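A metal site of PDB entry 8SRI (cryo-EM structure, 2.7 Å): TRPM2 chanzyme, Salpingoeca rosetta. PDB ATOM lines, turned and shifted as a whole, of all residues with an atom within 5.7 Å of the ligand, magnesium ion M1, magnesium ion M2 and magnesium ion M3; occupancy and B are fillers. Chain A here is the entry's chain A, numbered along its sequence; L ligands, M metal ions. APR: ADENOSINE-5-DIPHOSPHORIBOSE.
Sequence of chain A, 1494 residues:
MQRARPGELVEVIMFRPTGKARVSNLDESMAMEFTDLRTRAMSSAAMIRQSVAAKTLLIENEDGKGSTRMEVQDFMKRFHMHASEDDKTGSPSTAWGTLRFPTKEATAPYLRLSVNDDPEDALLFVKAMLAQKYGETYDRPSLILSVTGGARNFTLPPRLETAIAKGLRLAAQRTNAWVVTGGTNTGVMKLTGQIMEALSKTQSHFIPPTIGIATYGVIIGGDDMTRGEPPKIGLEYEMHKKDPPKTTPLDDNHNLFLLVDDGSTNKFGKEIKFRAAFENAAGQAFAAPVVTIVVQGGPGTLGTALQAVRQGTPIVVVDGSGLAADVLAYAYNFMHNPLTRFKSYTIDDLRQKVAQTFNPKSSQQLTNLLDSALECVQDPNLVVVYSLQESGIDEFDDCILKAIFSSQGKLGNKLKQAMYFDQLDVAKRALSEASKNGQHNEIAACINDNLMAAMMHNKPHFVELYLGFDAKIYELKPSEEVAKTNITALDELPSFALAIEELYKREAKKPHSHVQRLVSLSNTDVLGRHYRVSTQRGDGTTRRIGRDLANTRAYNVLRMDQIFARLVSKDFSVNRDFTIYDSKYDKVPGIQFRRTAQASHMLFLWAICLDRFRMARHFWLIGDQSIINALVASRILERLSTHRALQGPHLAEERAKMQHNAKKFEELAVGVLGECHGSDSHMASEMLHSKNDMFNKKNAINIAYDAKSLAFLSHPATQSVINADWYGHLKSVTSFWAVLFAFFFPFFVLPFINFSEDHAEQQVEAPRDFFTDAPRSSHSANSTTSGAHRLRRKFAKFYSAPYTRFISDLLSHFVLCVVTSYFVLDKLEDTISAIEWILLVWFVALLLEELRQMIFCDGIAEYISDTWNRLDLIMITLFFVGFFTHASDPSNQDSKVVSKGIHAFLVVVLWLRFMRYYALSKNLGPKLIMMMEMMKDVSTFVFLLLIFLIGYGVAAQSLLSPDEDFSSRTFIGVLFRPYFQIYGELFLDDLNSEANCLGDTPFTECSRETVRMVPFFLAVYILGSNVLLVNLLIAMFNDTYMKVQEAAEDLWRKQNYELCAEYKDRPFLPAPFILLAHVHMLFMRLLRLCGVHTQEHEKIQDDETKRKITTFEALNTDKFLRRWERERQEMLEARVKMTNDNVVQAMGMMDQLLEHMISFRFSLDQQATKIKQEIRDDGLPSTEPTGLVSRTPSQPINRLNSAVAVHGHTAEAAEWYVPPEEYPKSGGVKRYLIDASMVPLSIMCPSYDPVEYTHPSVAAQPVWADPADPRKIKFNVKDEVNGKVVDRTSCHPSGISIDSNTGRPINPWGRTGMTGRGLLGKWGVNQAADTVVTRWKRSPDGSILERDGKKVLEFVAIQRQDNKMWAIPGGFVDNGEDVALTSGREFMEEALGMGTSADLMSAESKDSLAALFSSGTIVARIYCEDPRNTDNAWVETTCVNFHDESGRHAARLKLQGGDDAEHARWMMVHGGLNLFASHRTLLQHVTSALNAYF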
ATOM      1  N   TRP A1264      29.004  -4.900 -19.733  1.00  0.00           N
ATOM      2  CA  TRP A1264      28.917  -4.554 -18.321  1.00  0.00           C
ATOM      3  C   TRP A1264      27.609  -4.995 -17.675  1.00  0.00           C
ATOM      4  O   TRP A1264      27.349  -4.642 -16.529  1.00  0.00           O
ATOM      5  CB  TRP A1264      29.078  -3.032 -18.135  1.00  0.00           C
ATOM      6  CG  TRP A1264      28.313  -2.186 -19.139  1.00  0.00           C
ATOM      7  CD1 TRP A1264      28.777  -1.694 -20.342  1.00  0.00           C
ATOM      8  CD2 TRP A1264      26.943  -1.755 -19.059  1.00  0.00           C
ATOM      9  NE1 TRP A1264      27.800  -0.984 -20.982  1.00  0.00           N
ATOM     10  CE2 TRP A1264      26.655  -1.005 -20.218  1.00  0.00           C
ATOM     11  CE3 TRP A1264      25.928  -1.930 -18.097  1.00  0.00           C
ATOM     12  CZ2 TRP A1264      25.404  -0.436 -20.453  1.00  0.00           C
ATOM     13  CZ3 TRP A1264      24.676  -1.357 -18.323  1.00  0.00           C
ATOM     14  CH2 TRP A1264      24.429  -0.616 -19.499  1.00  0.00           C
ATOM     15  N   LEU A1319      17.246   0.348 -15.330  1.00  0.00           N
ATOM     16  CA  LEU A1319      18.401   0.888 -16.028  1.00  0.00           C
ATOM     17  C   LEU A1319      19.726   0.328 -15.528  1.00  0.00           C
ATOM     18  O   LEU A1319      20.773   0.608 -16.142  1.00  0.00           O
ATOM     19  CB  LEU A1319      18.446   2.412 -15.891  1.00  0.00           C
ATOM     20  CG  LEU A1319      17.723   3.263 -16.937  1.00  0.00           C
ATOM     21  CD1 LEU A1319      17.587   4.683 -16.424  1.00  0.00           C
ATOM     22  CD2 LEU A1319      18.452   3.238 -18.267  1.00  0.00           C
ATOM     23  N   LEU A1320      19.728  -0.452 -14.457  1.00  0.00           N
ATOM     24  CA  LEU A1320      20.948  -0.974 -13.869  1.00  0.00           C
ATOM     25  C   LEU A1320      21.297  -2.314 -14.505  1.00  0.00           C
ATOM     26  O   LEU A1320      20.425  -3.172 -14.689  1.00  0.00           O
ATOM     27  CB  LEU A1320      20.802  -1.097 -12.353  1.00  0.00           C
ATOM     28  CG  LEU A1320      20.505   0.209 -11.619  1.00  0.00           C
ATOM     29  CD1 LEU A1320      20.384  -0.029 -10.126  1.00  0.00           C
ATOM     30  CD2 LEU A1320      21.567   1.271 -11.886  1.00  0.00           C
ATOM     31  N   GLY A1321      22.573  -2.501 -14.822  1.00  0.00           N
ATOM     32  CA  GLY A1321      23.000  -3.658 -15.590  1.00  0.00           C
ATOM     33  C   GLY A1321      23.277  -4.906 -14.780  1.00  0.00           C
ATOM     34  O   GLY A1321      23.240  -6.008 -15.325  1.00  0.00           O
ATOM     35  N   LYS A1322      23.550  -4.752 -13.486  1.00  0.00           N
ATOM     36  CA  LYS A1322      23.952  -5.870 -12.640  1.00  0.00           C
ATOM     37  C   LYS A1322      22.876  -6.165 -11.609  1.00  0.00           C
ATOM     38  O   LYS A1322      22.300  -5.239 -11.023  1.00  0.00           O
ATOM     39  CB  LYS A1322      25.285  -5.571 -11.945  1.00  0.00           C
ATOM     40  N   ASN A1326      24.886  -2.776  -7.080  1.00  0.00           N
ATOM     41  CA  ASN A1326      25.754  -2.056  -7.992  1.00  0.00           C
ATOM     42  C   ASN A1326      26.673  -1.188  -7.142  1.00  0.00           C
ATOM     43  O   ASN A1326      26.227  -0.217  -6.523  1.00  0.00           O
ATOM     44  CB  ASN A1326      24.946  -1.191  -8.951  1.00  0.00           C
ATOM     45  CG  ASN A1326      24.320  -1.992 -10.074  1.00  0.00           C
ATOM     46  OD1 ASN A1326      24.990  -2.336 -11.044  1.00  0.00           O
ATOM     47  ND2 ASN A1326      23.042  -2.300  -9.937  1.00  0.00           N
ATOM     48  N   ALA A1328      29.124   1.583  -6.538  1.00  0.00           N
ATOM     49  CA  ALA A1328      29.536   2.827  -7.154  1.00  0.00           C
ATOM     50  C   ALA A1328      30.635   3.461  -6.332  1.00  0.00           C
ATOM     51  O   ALA A1328      30.715   3.253  -5.115  1.00  0.00           O
ATOM     52  CB  ALA A1328      28.357   3.798  -7.280  1.00  0.00           C
ATOM     53  N   ALA A1329      31.508   4.198  -7.006  1.00  0.00           N
ATOM     54  CA  ALA A1329      32.563   4.932  -6.336  1.00  0.00           C
ATOM     55  C   ALA A1329      32.383   6.408  -6.638  1.00  0.00           C
ATOM     56  O   ALA A1329      32.218   6.797  -7.805  1.00  0.00           O
ATOM     57  CB  ALA A1329      33.947   4.473  -6.809  1.00  0.00           C
ATOM     58  N   ASP A1330      32.382   7.220  -5.583  1.00  0.00           N
ATOM     59  CA  ASP A1330      32.288   8.658  -5.698  1.00  0.00           C
ATOM     60  C   ASP A1330      33.584   9.313  -5.243  1.00  0.00           C
ATOM     61  O   ASP A1330      34.211   8.878  -4.270  1.00  0.00           O
ATOM     62  CB  ASP A1330      31.107   9.194  -4.892  1.00  0.00           C
ATOM     63  CG  ASP A1330      29.783   8.686  -5.419  1.00  0.00           C
ATOM     64  OD1 ASP A1330      29.557   8.774  -6.645  1.00  0.00           O
ATOM     65  OD2 ASP A1330      28.964   8.187  -4.623  1.00  0.00           O
ATOM     66  N   ILE A1358      29.655  18.177 -10.825  1.00  0.00           N
ATOM     67  CA  ILE A1358      29.351  18.033 -12.251  1.00  0.00           C
ATOM     68  C   ILE A1358      27.844  18.067 -12.497  1.00  0.00           C
ATOM     69  O   ILE A1358      27.037  17.708 -11.631  1.00  0.00           O
ATOM     70  CB  ILE A1358      30.012  16.767 -12.854  1.00  0.00           C
ATOM     71  CG1 ILE A1358      29.457  15.486 -12.222  1.00  0.00           C
ATOM     72  CG2 ILE A1358      31.532  16.890 -12.831  1.00  0.00           C
ATOM     73  CD1 ILE A1358      29.496  14.271 -13.086  1.00  0.00           C
ATOM     74  N   ARG A1360      24.875  16.553 -14.529  1.00  0.00           N
ATOM     75  CA  ARG A1360      24.518  15.295 -15.196  1.00  0.00           C
ATOM     76  C   ARG A1360      23.815  15.516 -16.534  1.00  0.00           C
ATOM     77  O   ARG A1360      23.102  16.509 -16.718  1.00  0.00           O
ATOM     78  CB  ARG A1360      23.653  14.438 -14.280  1.00  0.00           C
ATOM     79  CG  ARG A1360      24.312  14.111 -12.951  1.00  0.00           C
ATOM     80  CD  ARG A1360      23.420  13.243 -12.074  1.00  0.00           C
ATOM     81  NE  ARG A1360      22.937  12.057 -12.772  1.00  0.00           N
ATOM     82  CZ  ARG A1360      23.599  10.907 -12.844  1.00  0.00           C
ATOM     83  NH1 ARG A1360      24.777  10.742 -12.274  1.00  0.00           N
ATOM     84  NH2 ARG A1360      23.052   9.886 -13.506  1.00  0.00           N
ATOM     85  N   ILE A1368      28.020  14.784  -7.400  1.00  0.00           N
ATOM     86  CA  ILE A1368      29.423  14.394  -7.197  1.00  0.00           C
ATOM     87  C   ILE A1368      29.844  13.464  -8.328  1.00  0.00           C
ATOM     88  O   ILE A1368      29.002  12.651  -8.780  1.00  0.00           O
ATOM     89  CB  ILE A1368      29.590  13.718  -5.815  1.00  0.00           C
ATOM     90  CG1 ILE A1368      29.442  14.727  -4.675  1.00  0.00           C
ATOM     91  CG2 ILE A1368      30.903  12.946  -5.602  1.00  0.00           C
ATOM     92  CD1 ILE A1368      29.243  14.122  -3.315  1.00  0.00           C
ATOM     93  N   PRO A1369      31.039  13.679  -8.945  1.00  0.00           N
ATOM     94  CA  PRO A1369      31.563  12.737  -9.962  1.00  0.00           C
ATOM     95  C   PRO A1369      31.780  11.330  -9.418  1.00  0.00           C
ATOM     96  O   PRO A1369      32.218  11.146  -8.275  1.00  0.00           O
ATOM     97  CB  PRO A1369      32.914  13.367 -10.353  1.00  0.00           C
ATOM     98  CG  PRO A1369      32.816  14.773  -9.971  1.00  0.00           C
ATOM     99  CD  PRO A1369      31.927  14.836  -8.778  1.00  0.00           C
ATOM    100  N   GLY A1370      31.466  10.335 -10.236  1.00  0.00           N
ATOM    101  CA  GLY A1370      31.611   8.959  -9.801  1.00  0.00           C
ATOM    102  C   GLY A1370      30.917   8.016 -10.762  1.00  0.00           C
ATOM    103  O   GLY A1370      30.227   8.448 -11.695  1.00  0.00           O
ATOM    104  N   GLY A1371      31.110   6.732 -10.515  1.00  0.00           N
ATOM    105  CA  GLY A1371      30.521   5.759 -11.418  1.00  0.00           C
ATOM    106  C   GLY A1371      30.631   4.325 -10.944  1.00  0.00           C
ATOM    107  O   GLY A1371      31.220   4.022  -9.901  1.00  0.00           O
ATOM    108  N   PHE A1372      29.980   3.461 -11.728  1.00  0.00           N
ATOM    109  CA  PHE A1372      29.883   2.023 -11.464  1.00  0.00           C
ATOM    110  C   PHE A1372      31.248   1.354 -11.654  1.00  0.00           C
ATOM    111  O   PHE A1372      32.026   1.734 -12.528  1.00  0.00           O
ATOM    112  CB  PHE A1372      28.831   1.418 -12.378  1.00  0.00           C
ATOM    113  CG  PHE A1372      27.442   1.926 -12.103  1.00  0.00           C
ATOM    114  CD1 PHE A1372      26.754   1.518 -10.950  1.00  0.00           C
ATOM    115  CD2 PHE A1372      26.863   2.884 -12.956  1.00  0.00           C
ATOM    116  CE1 PHE A1372      25.466   2.018 -10.678  1.00  0.00           C
ATOM    117  CE2 PHE A1372      25.585   3.394 -12.686  1.00  0.00           C
ATOM    118  CZ  PHE A1372      24.887   2.961 -11.547  1.00  0.00           C
ATOM    119  N   VAL A1373      31.536   0.359 -10.814  1.00  0.00           N
ATOM    120  CA  VAL A1373      32.812  -0.368 -10.914  1.00  0.00           C
ATOM    121  C   VAL A1373      32.854  -1.331 -12.096  1.00  0.00           C
ATOM    122  O   VAL A1373      31.919  -2.110 -12.342  1.00  0.00           O
ATOM    123  CB  VAL A1373      33.202  -1.030  -9.568  1.00  0.00           C
ATOM    124  CG1 VAL A1373      33.466   0.044  -8.526  1.00  0.00           C
ATOM    125  CG2 VAL A1373      32.195  -2.033  -9.022  1.00  0.00           C
ATOM    126  N   ARG A1385      39.487   7.323 -12.341  1.00  0.00           N
ATOM    127  CA  ARG A1385      39.168   7.262 -13.775  1.00  0.00           C
ATOM    128  C   ARG A1385      37.914   8.088 -14.098  1.00  0.00           C
ATOM    129  O   ARG A1385      37.885   8.794 -15.113  1.00  0.00           O
ATOM    130  CB  ARG A1385      39.016   5.802 -14.215  1.00  0.00           C
ATOM    131  CG  ARG A1385      38.754   5.590 -15.710  1.00  0.00           C
ATOM    132  CD  ARG A1385      38.537   4.117 -16.075  1.00  0.00           C
ATOM    133  NE  ARG A1385      37.659   3.397 -15.164  1.00  0.00           N
ATOM    134  CZ  ARG A1385      36.328   3.398 -15.220  1.00  0.00           C
ATOM    135  NH1 ARG A1385      35.670   4.088 -16.134  1.00  0.00           N
ATOM    136  NH2 ARG A1385      35.643   2.675 -14.341  1.00  0.00           N
ATOM    137  N   GLU A1386      36.869   7.961 -13.250  1.00  0.00           N
ATOM    138  CA  GLU A1386      35.632   8.739 -13.398  1.00  0.00           C
ATOM    139  C   GLU A1386      35.887  10.226 -13.142  1.00  0.00           C
ATOM    140  O   GLU A1386      35.173  11.052 -13.724  1.00  0.00           O
ATOM    141  CB  GLU A1386      34.485   8.229 -12.519  1.00  0.00           C
ATOM    142  CG  GLU A1386      33.835   6.878 -12.926  1.00  0.00           C
ATOM    143  CD  GLU A1386      33.366   6.790 -14.379  1.00  0.00           C
ATOM    144  OE1 GLU A1386      32.764   7.757 -14.898  1.00  0.00           O
ATOM    145  OE2 GLU A1386      33.607   5.737 -15.002  1.00  0.00           O
ATOM    146  N   GLU A1390      35.039  12.616 -16.169  1.00  0.00           N
ATOM    147  CA  GLU A1390      33.867  13.474 -16.034  1.00  0.00           C
ATOM    148  C   GLU A1390      34.207  14.931 -15.721  1.00  0.00           C
ATOM    149  O   GLU A1390      33.766  15.836 -16.422  1.00  0.00           O
ATOM    150  CB  GLU A1390      32.935  12.871 -14.975  1.00  0.00           C
ATOM    151  CG  GLU A1390      32.308  11.542 -15.409  1.00  0.00           C
ATOM    152  CD  GLU A1390      31.416  10.937 -14.348  1.00  0.00           C
ATOM    153  OE1 GLU A1390      31.376  11.460 -13.217  1.00  0.00           O
ATOM    154  OE2 GLU A1390      30.726   9.940 -14.655  1.00  0.00           O
ATOM    155  N   CYS A1424      22.571   4.144  -1.487  1.00  0.00           N
ATOM    156  CA  CYS A1424      22.084   5.320  -2.210  1.00  0.00           C
ATOM    157  C   CYS A1424      20.566   5.400  -2.259  1.00  0.00           C
ATOM    158  O   CYS A1424      19.891   4.393  -2.499  1.00  0.00           O
ATOM    159  CB  CYS A1424      22.562   5.332  -3.671  1.00  0.00           C
ATOM    160  SG  CYS A1424      24.276   5.656  -4.013  1.00  0.00           S
ATOM    161  N   ASP A1426      18.913   6.634  -4.742  1.00  0.00           N
ATOM    162  CA  ASP A1426      18.988   6.830  -6.180  1.00  0.00           C
ATOM    163  C   ASP A1426      17.630   6.514  -6.806  1.00  0.00           C
ATOM    164  O   ASP A1426      17.046   5.483  -6.473  1.00  0.00           O
ATOM    165  CB  ASP A1426      20.073   5.889  -6.736  1.00  0.00           C
ATOM    166  CG  ASP A1426      20.514   6.213  -8.157  1.00  0.00           C
ATOM    167  OD1 ASP A1426      19.748   6.031  -9.138  1.00  0.00           O
ATOM    168  OD2 ASP A1426      21.688   6.618  -8.311  1.00  0.00           O
ATOM    169  N   ARG A1428      16.786   5.522  -9.789  1.00  0.00           N
ATOM    170  CA  ARG A1428      16.803   4.397 -10.705  1.00  0.00           C
ATOM    171  C   ARG A1428      16.772   3.037 -10.009  1.00  0.00           C
ATOM    172  O   ARG A1428      16.799   2.013 -10.716  1.00  0.00           O
ATOM    173  CB  ARG A1428      18.040   4.457 -11.616  1.00  0.00           C
ATOM    174  CG  ARG A1428      18.204   5.763 -12.382  1.00  0.00           C
ATOM    175  CD  ARG A1428      19.611   5.892 -12.927  1.00  0.00           C
ATOM    176  NE  ARG A1428      20.587   6.156 -11.879  1.00  0.00           N
ATOM    177  CZ  ARG A1428      21.885   6.352 -12.093  1.00  0.00           C
ATOM    178  NH1 ARG A1428      22.396   6.328 -13.308  1.00  0.00           N
ATOM    179  NH2 ARG A1428      22.690   6.583 -11.053  1.00  0.00           N
ATOM    180  N   VAL A1435      21.851   0.665  -6.016  1.00  0.00           N
ATOM    181  CA  VAL A1435      23.183   1.268  -5.986  1.00  0.00           C
ATOM    182  C   VAL A1435      23.648   1.461  -4.537  1.00  0.00           C
ATOM    183  O   VAL A1435      22.895   1.976  -3.703  1.00  0.00           O
ATOM    184  CB  VAL A1435      23.177   2.608  -6.751  1.00  0.00           C
ATOM    185  CG1 VAL A1435      24.569   3.220  -6.870  1.00  0.00           C
ATOM    186  CG2 VAL A1435      22.588   2.412  -8.141  1.00  0.00           C
ATOM    187  N   THR A1437      27.179   2.973  -2.519  1.00  0.00           N
ATOM    188  CA  THR A1437      28.335   3.802  -2.861  1.00  0.00           C
ATOM    189  C   THR A1437      29.434   3.700  -1.808  1.00  0.00           C
ATOM    190  O   THR A1437      29.183   3.441  -0.622  1.00  0.00           O
ATOM    191  CB  THR A1437      27.959   5.292  -3.071  1.00  0.00           C
ATOM    192  OG1 THR A1437      29.146   6.037  -3.340  1.00  0.00           O
ATOM    193  CG2 THR A1437      27.286   5.934  -1.843  1.00  0.00           C
ATOM    194  N   ASP A1459      32.534  13.369 -20.973  1.00  0.00           N
ATOM    195  CA  ASP A1459      31.786  12.101 -20.905  1.00  0.00           C
ATOM    196  C   ASP A1459      30.306  12.373 -20.627  1.00  0.00           C
ATOM    197  O   ASP A1459      29.627  12.992 -21.444  1.00  0.00           O
ATOM    198  CB  ASP A1459      32.405  11.142 -19.891  1.00  0.00           C
ATOM    199  N   ASP A1460      29.835  11.914 -19.457  1.00  0.00           N
ATOM    200  CA  ASP A1460      28.401  12.051 -19.068  1.00  0.00           C
ATOM    201  C   ASP A1460      28.209  13.270 -18.161  1.00  0.00           C
ATOM    202  O   ASP A1460      27.327  13.222 -17.300  1.00  0.00           O
ATOM    203  CB  ASP A1460      27.884  10.781 -18.395  1.00  0.00           C
ATOM    204  CG  ASP A1460      28.727  10.299 -17.236  1.00  0.00           C
ATOM    205  OD1 ASP A1460      29.723   9.594 -17.486  1.00  0.00           O
ATOM    206  OD2 ASP A1460      28.376  10.628 -16.086  1.00  0.00           O
ATOM    207  N   PHE A1476      21.921  15.083  -6.599  1.00  0.00           N
ATOM    208  CA  PHE A1476      21.397  13.796  -7.043  1.00  0.00           C
ATOM    209  C   PHE A1476      21.729  12.739  -5.999  1.00  0.00           C
ATOM    210  O   PHE A1476      22.848  12.744  -5.469  1.00  0.00           O
ATOM    211  CB  PHE A1476      22.004  13.469  -8.414  1.00  0.00           C
ATOM    212  CG  PHE A1476      21.768  12.079  -8.882  1.00  0.00           C
ATOM    213  CD1 PHE A1476      20.476  11.662  -9.227  1.00  0.00           C
ATOM    214  CD2 PHE A1476      22.849  11.187  -9.042  1.00  0.00           C
ATOM    215  CE1 PHE A1476      20.234  10.368  -9.696  1.00  0.00           C
ATOM    216  CE2 PHE A1476      22.626   9.882  -9.506  1.00  0.00           C
ATOM    217  CZ  PHE A1476      21.315   9.482  -9.837  1.00  0.00           C
ATOM    218  N   ALA A1477      20.775  11.821  -5.754  1.00  0.00           N
ATOM    219  CA  ALA A1477      20.820  10.610  -4.883  1.00  0.00           C
ATOM    220  C   ALA A1477      21.165  11.011  -3.437  1.00  0.00           C
ATOM    221  O   ALA A1477      20.575  11.966  -2.925  1.00  0.00           O
ATOM    222  CB  ALA A1477      21.734   9.550  -5.512  1.00  0.00           C
ATOM    223  N   HIS A1479      24.071  12.243  -2.190  1.00  0.00           N
ATOM    224  CA  HIS A1479      25.321  13.009  -2.167  1.00  0.00           C
ATOM    225  C   HIS A1479      25.388  14.068  -1.055  1.00  0.00           C
ATOM    226  O   HIS A1479      26.499  14.478  -0.706  1.00  0.00           O
ATOM    227  CB  HIS A1479      25.512  13.618  -3.550  1.00  0.00           C
ATOM    228  CG  HIS A1479      25.894  12.613  -4.595  1.00  0.00           C
ATOM    229  ND1 HIS A1479      25.997  12.929  -5.925  1.00  0.00           N
ATOM    230  CD2 HIS A1479      26.205  11.294  -4.489  1.00  0.00           C
ATOM    231  CE1 HIS A1479      26.342  11.858  -6.611  1.00  0.00           C
ATOM    232  NE2 HIS A1479      26.478  10.845  -5.761  1.00  0.00           N
ATOM    233  N   LEU A1482      26.824  12.168   1.792  1.00  0.00           N
ATOM    234  CA  LEU A1482      28.260  12.024   1.510  1.00  0.00           C
ATOM    235  C   LEU A1482      29.042  13.298   1.844  1.00  0.00           C
ATOM    236  O   LEU A1482      30.145  13.232   2.409  1.00  0.00           O
ATOM    237  CB  LEU A1482      28.460  11.641   0.043  1.00  0.00           C
ATOM    238  CG  LEU A1482      27.918  10.263  -0.359  1.00  0.00           C
ATOM    239  CD1 LEU A1482      28.271   9.971  -1.808  1.00  0.00           C
ATOM    240  CD2 LEU A1482      28.405   9.129   0.549  1.00  0.00           C
HETATM  241  N1  APR L   1      24.558  -0.061 -14.234  1.00  0.00           N
HETATM  242  C2  APR L   1      24.178   0.929 -15.046  1.00  0.00           C
HETATM  243  N3  APR L   1      24.988   1.519 -15.947  1.00  0.00           N
HETATM  244  C4  APR L   1      26.274   1.124 -16.097  1.00  0.00           C
HETATM  245  C5  APR L   1      26.756   0.037 -15.237  1.00  0.00           C
HETATM  246  C6  APR L   1      25.811  -0.556 -14.277  1.00  0.00           C
HETATM  247  N6  APR L   1      26.190  -1.565 -13.459  1.00  0.00           N
HETATM  248  N7  APR L   1      28.042  -0.172 -15.556  1.00  0.00           N
HETATM  249  C8  APR L   1      28.359   0.701 -16.537  1.00  0.00           C
HETATM  250  N9  APR L   1      27.315   1.478 -16.865  1.00  0.00           N
HETATM  251  C1' APR L   1      27.415   2.523 -17.915  1.00  0.00           C
HETATM  252  C2' APR L   1      26.068   2.912 -18.517  1.00  0.00           C
HETATM  253  O2' APR L   1      26.111   2.689 -19.920  1.00  0.00           O
HETATM  254  C3' APR L   1      25.911   4.387 -18.256  1.00  0.00           C
HETATM  255  O3' APR L   1      25.408   5.046 -19.416  1.00  0.00           O
HETATM  256  O4' APR L   1      27.980   3.730 -17.389  1.00  0.00           O
HETATM  257  C4' APR L   1      27.319   4.855 -17.954  1.00  0.00           C
HETATM  258  C5' APR L   1      27.334   6.052 -17.008  1.00  0.00           C
HETATM  259  O5' APR L   1      28.629   6.200 -16.455  1.00  0.00           O
HETATM  260  PA  APR L   1      28.765   6.223 -14.858  1.00  0.00           P
HETATM  261  O1A APR L   1      29.689   7.354 -14.511  1.00  0.00           O
HETATM  262  O2A APR L   1      29.088   4.819 -14.405  1.00  0.00           O
HETATM  263  O3A APR L   1      27.238   6.567 -14.439  1.00  0.00           O
HETATM  264  PB  APR L   1      26.814   7.634 -13.311  1.00  0.00           P
HETATM  265  O1B APR L   1      25.308   7.669 -13.272  1.00  0.00           O
HETATM  266  O2B APR L   1      27.581   8.923 -13.502  1.00  0.00           O
HETATM  267  O5D APR L   1      27.323   6.944 -11.961  1.00  0.00           O
HETATM  268  C5D APR L   1      26.384   6.490 -10.996  1.00  0.00           C
HETATM  269  O4D APR L   1      24.872   7.359  -9.336  1.00  0.00           O
HETATM  270  O1D APR L   1      24.181   6.518  -7.243  1.00  0.00           O
HETATM  271  C1D APR L   1      25.004   7.469  -7.918  1.00  0.00           C
HETATM  272  O2D APR L   1      26.868   7.920  -6.509  1.00  0.00           O
HETATM  273  C2D APR L   1      26.455   7.166  -7.637  1.00  0.00           C
HETATM  274  O3D APR L   1      27.655   8.927  -8.718  1.00  0.00           O
HETATM  275  C3D APR L   1      27.181   7.591  -8.888  1.00  0.00           C
HETATM  276  C4D APR L   1      26.119   7.584  -9.975  1.00  0.00           C
HETATM  277 MG    MG M   1      30.810   8.202 -16.120  1.00  0.00          MG
HETATM  278 MG    MG M   2      29.276  10.036 -13.142  1.00  0.00          MG
HETATM  279 MG    MG M   3      30.932   6.093 -16.166  1.00  0.00          MG
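Magnesium ion M2 is bound by O2B of the ligand (2.1 Å), OE2 of Glu 1390 (2.1 Å), O of Gly 1370 (2.3 Å) and OE1 of Glu 1390 (2.5 Å).
Two residues have an atom within 4 Å of magnesium ion M3: Glu 1386 and Asp 1460.
OD2 of Asp 1426 sits at hydrogen-bond distance from O1D of the ligand, at 2.7 Å.
The side-chain amide oxygen (OD1) of Asn 1326 is in hydrogen-bond range of a nitrogen (N6) of the ligand, 2.8 Å away.
The side-chain carboxylate of Asp 1330 lies within hydrogen-bond range of an oxygen (O3D) of the ligand, at 2.8 Å.
O1B of the ligand is in salt-bridge range of NH1 of Arg 1428, at 3.2 Å.
A ring nitrogen (NE2) of His 1479 is in hydrogen-bond range of an oxygen (O2D) of the ligand.
N of Phe 1372 is in hydrogen-bond range of O2A of the ligand.
NH2 of Arg 1360 is in salt-bridge range of O1B of the ligand, at 3.2 Å.
The backbone NH (N) of Gly 1321 sits at hydrogen-bond distance from a nitrogen (N1) of the ligand (3.2 Å).
An oxygen (O1D) of the ligand lies within hydrogen-bond range of the side-chain sulfur (SG) of Cys 1424, 3.3 Å away.
Trp 1264 touches the ligand.
Leu 1319 touches the ligand (O to C2, 3.6 Å).
CA of Leu 1320 touches N1 of the ligand (3.7 Å).
Ala 1328 touches the ligand.
O of Ile 1368 touches O3D of the ligand, at 3.96 Å.
Gly 1371 touches the ligand (CA to O2A, 3.4 Å).
Val 1435 touches the ligand.
CE2 of Phe 1476 touches O4D of the ligand (3.4 Å).
Hydrophobic or aromatic side chains that line the ligand: Trp 1264, Ala 1328, Phe 1372, Val 1435, Phe 1476 and His 1479.
The nearest printed residue that does not touch the ligand is Lys 1322 (4.1 Å).
Magnesium ion M1 is bound by an oxygen (O1A) of the ligand (2.1 Å), the side-chain carboxylate of Asp 1460 (2.2 Å), the side-chain carboxylate of Glu 1390 (2.3 Å) and the side-chain carboxylate of Glu 1386 (2.3 Å).
Magnesium ion M1 has four donor atoms within binding distance.
Magnesium ion M3 is bound by O5' of the ligand (2.3 Å) and O1A of the ligand (2.4 Å).
Slightly farther from magnesium ion M3 lies OE1 of Glu 1386 (2.8 Å).
Within 4 Å of magnesium ion M2: Gly 1370, Glu 1390 and Asp 1460.
OE2 of Glu 1386 is in salt-bridge range of NH1 of Arg 1385, at 2.9 Å.
The guanidinium group (NE) of Arg 1428 is in salt-bridge range of the side-chain carboxylate (OD1) of Asp 1426 (2.9 Å).
The side-chain amide nitrogen (ND2) of Asn 1326 is in hydrogen-bond range of the backbone carbonyl oxygen (O) of Lys 1322 (3.2 Å).
OG1 of Thr 1437 lies within hydrogen-bond range of OD2 of Asp 1330 (2.5 Å).
A ring nitrogen (ND1) of His 1479 lies close to the backbone carbonyl oxygen (O) of Phe 1476 (3.2 Å).
N of Ile 1368 is in hydrogen-bond range of ND1 of His 1479, at 3.1 Å.
N of Cys 1424 lies within hydrogen-bond range of O of Val 1435 (3.1 Å).
O of Gly 1371 lies within hydrogen-bond range of N of Ala 1329, at 2.9 Å.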
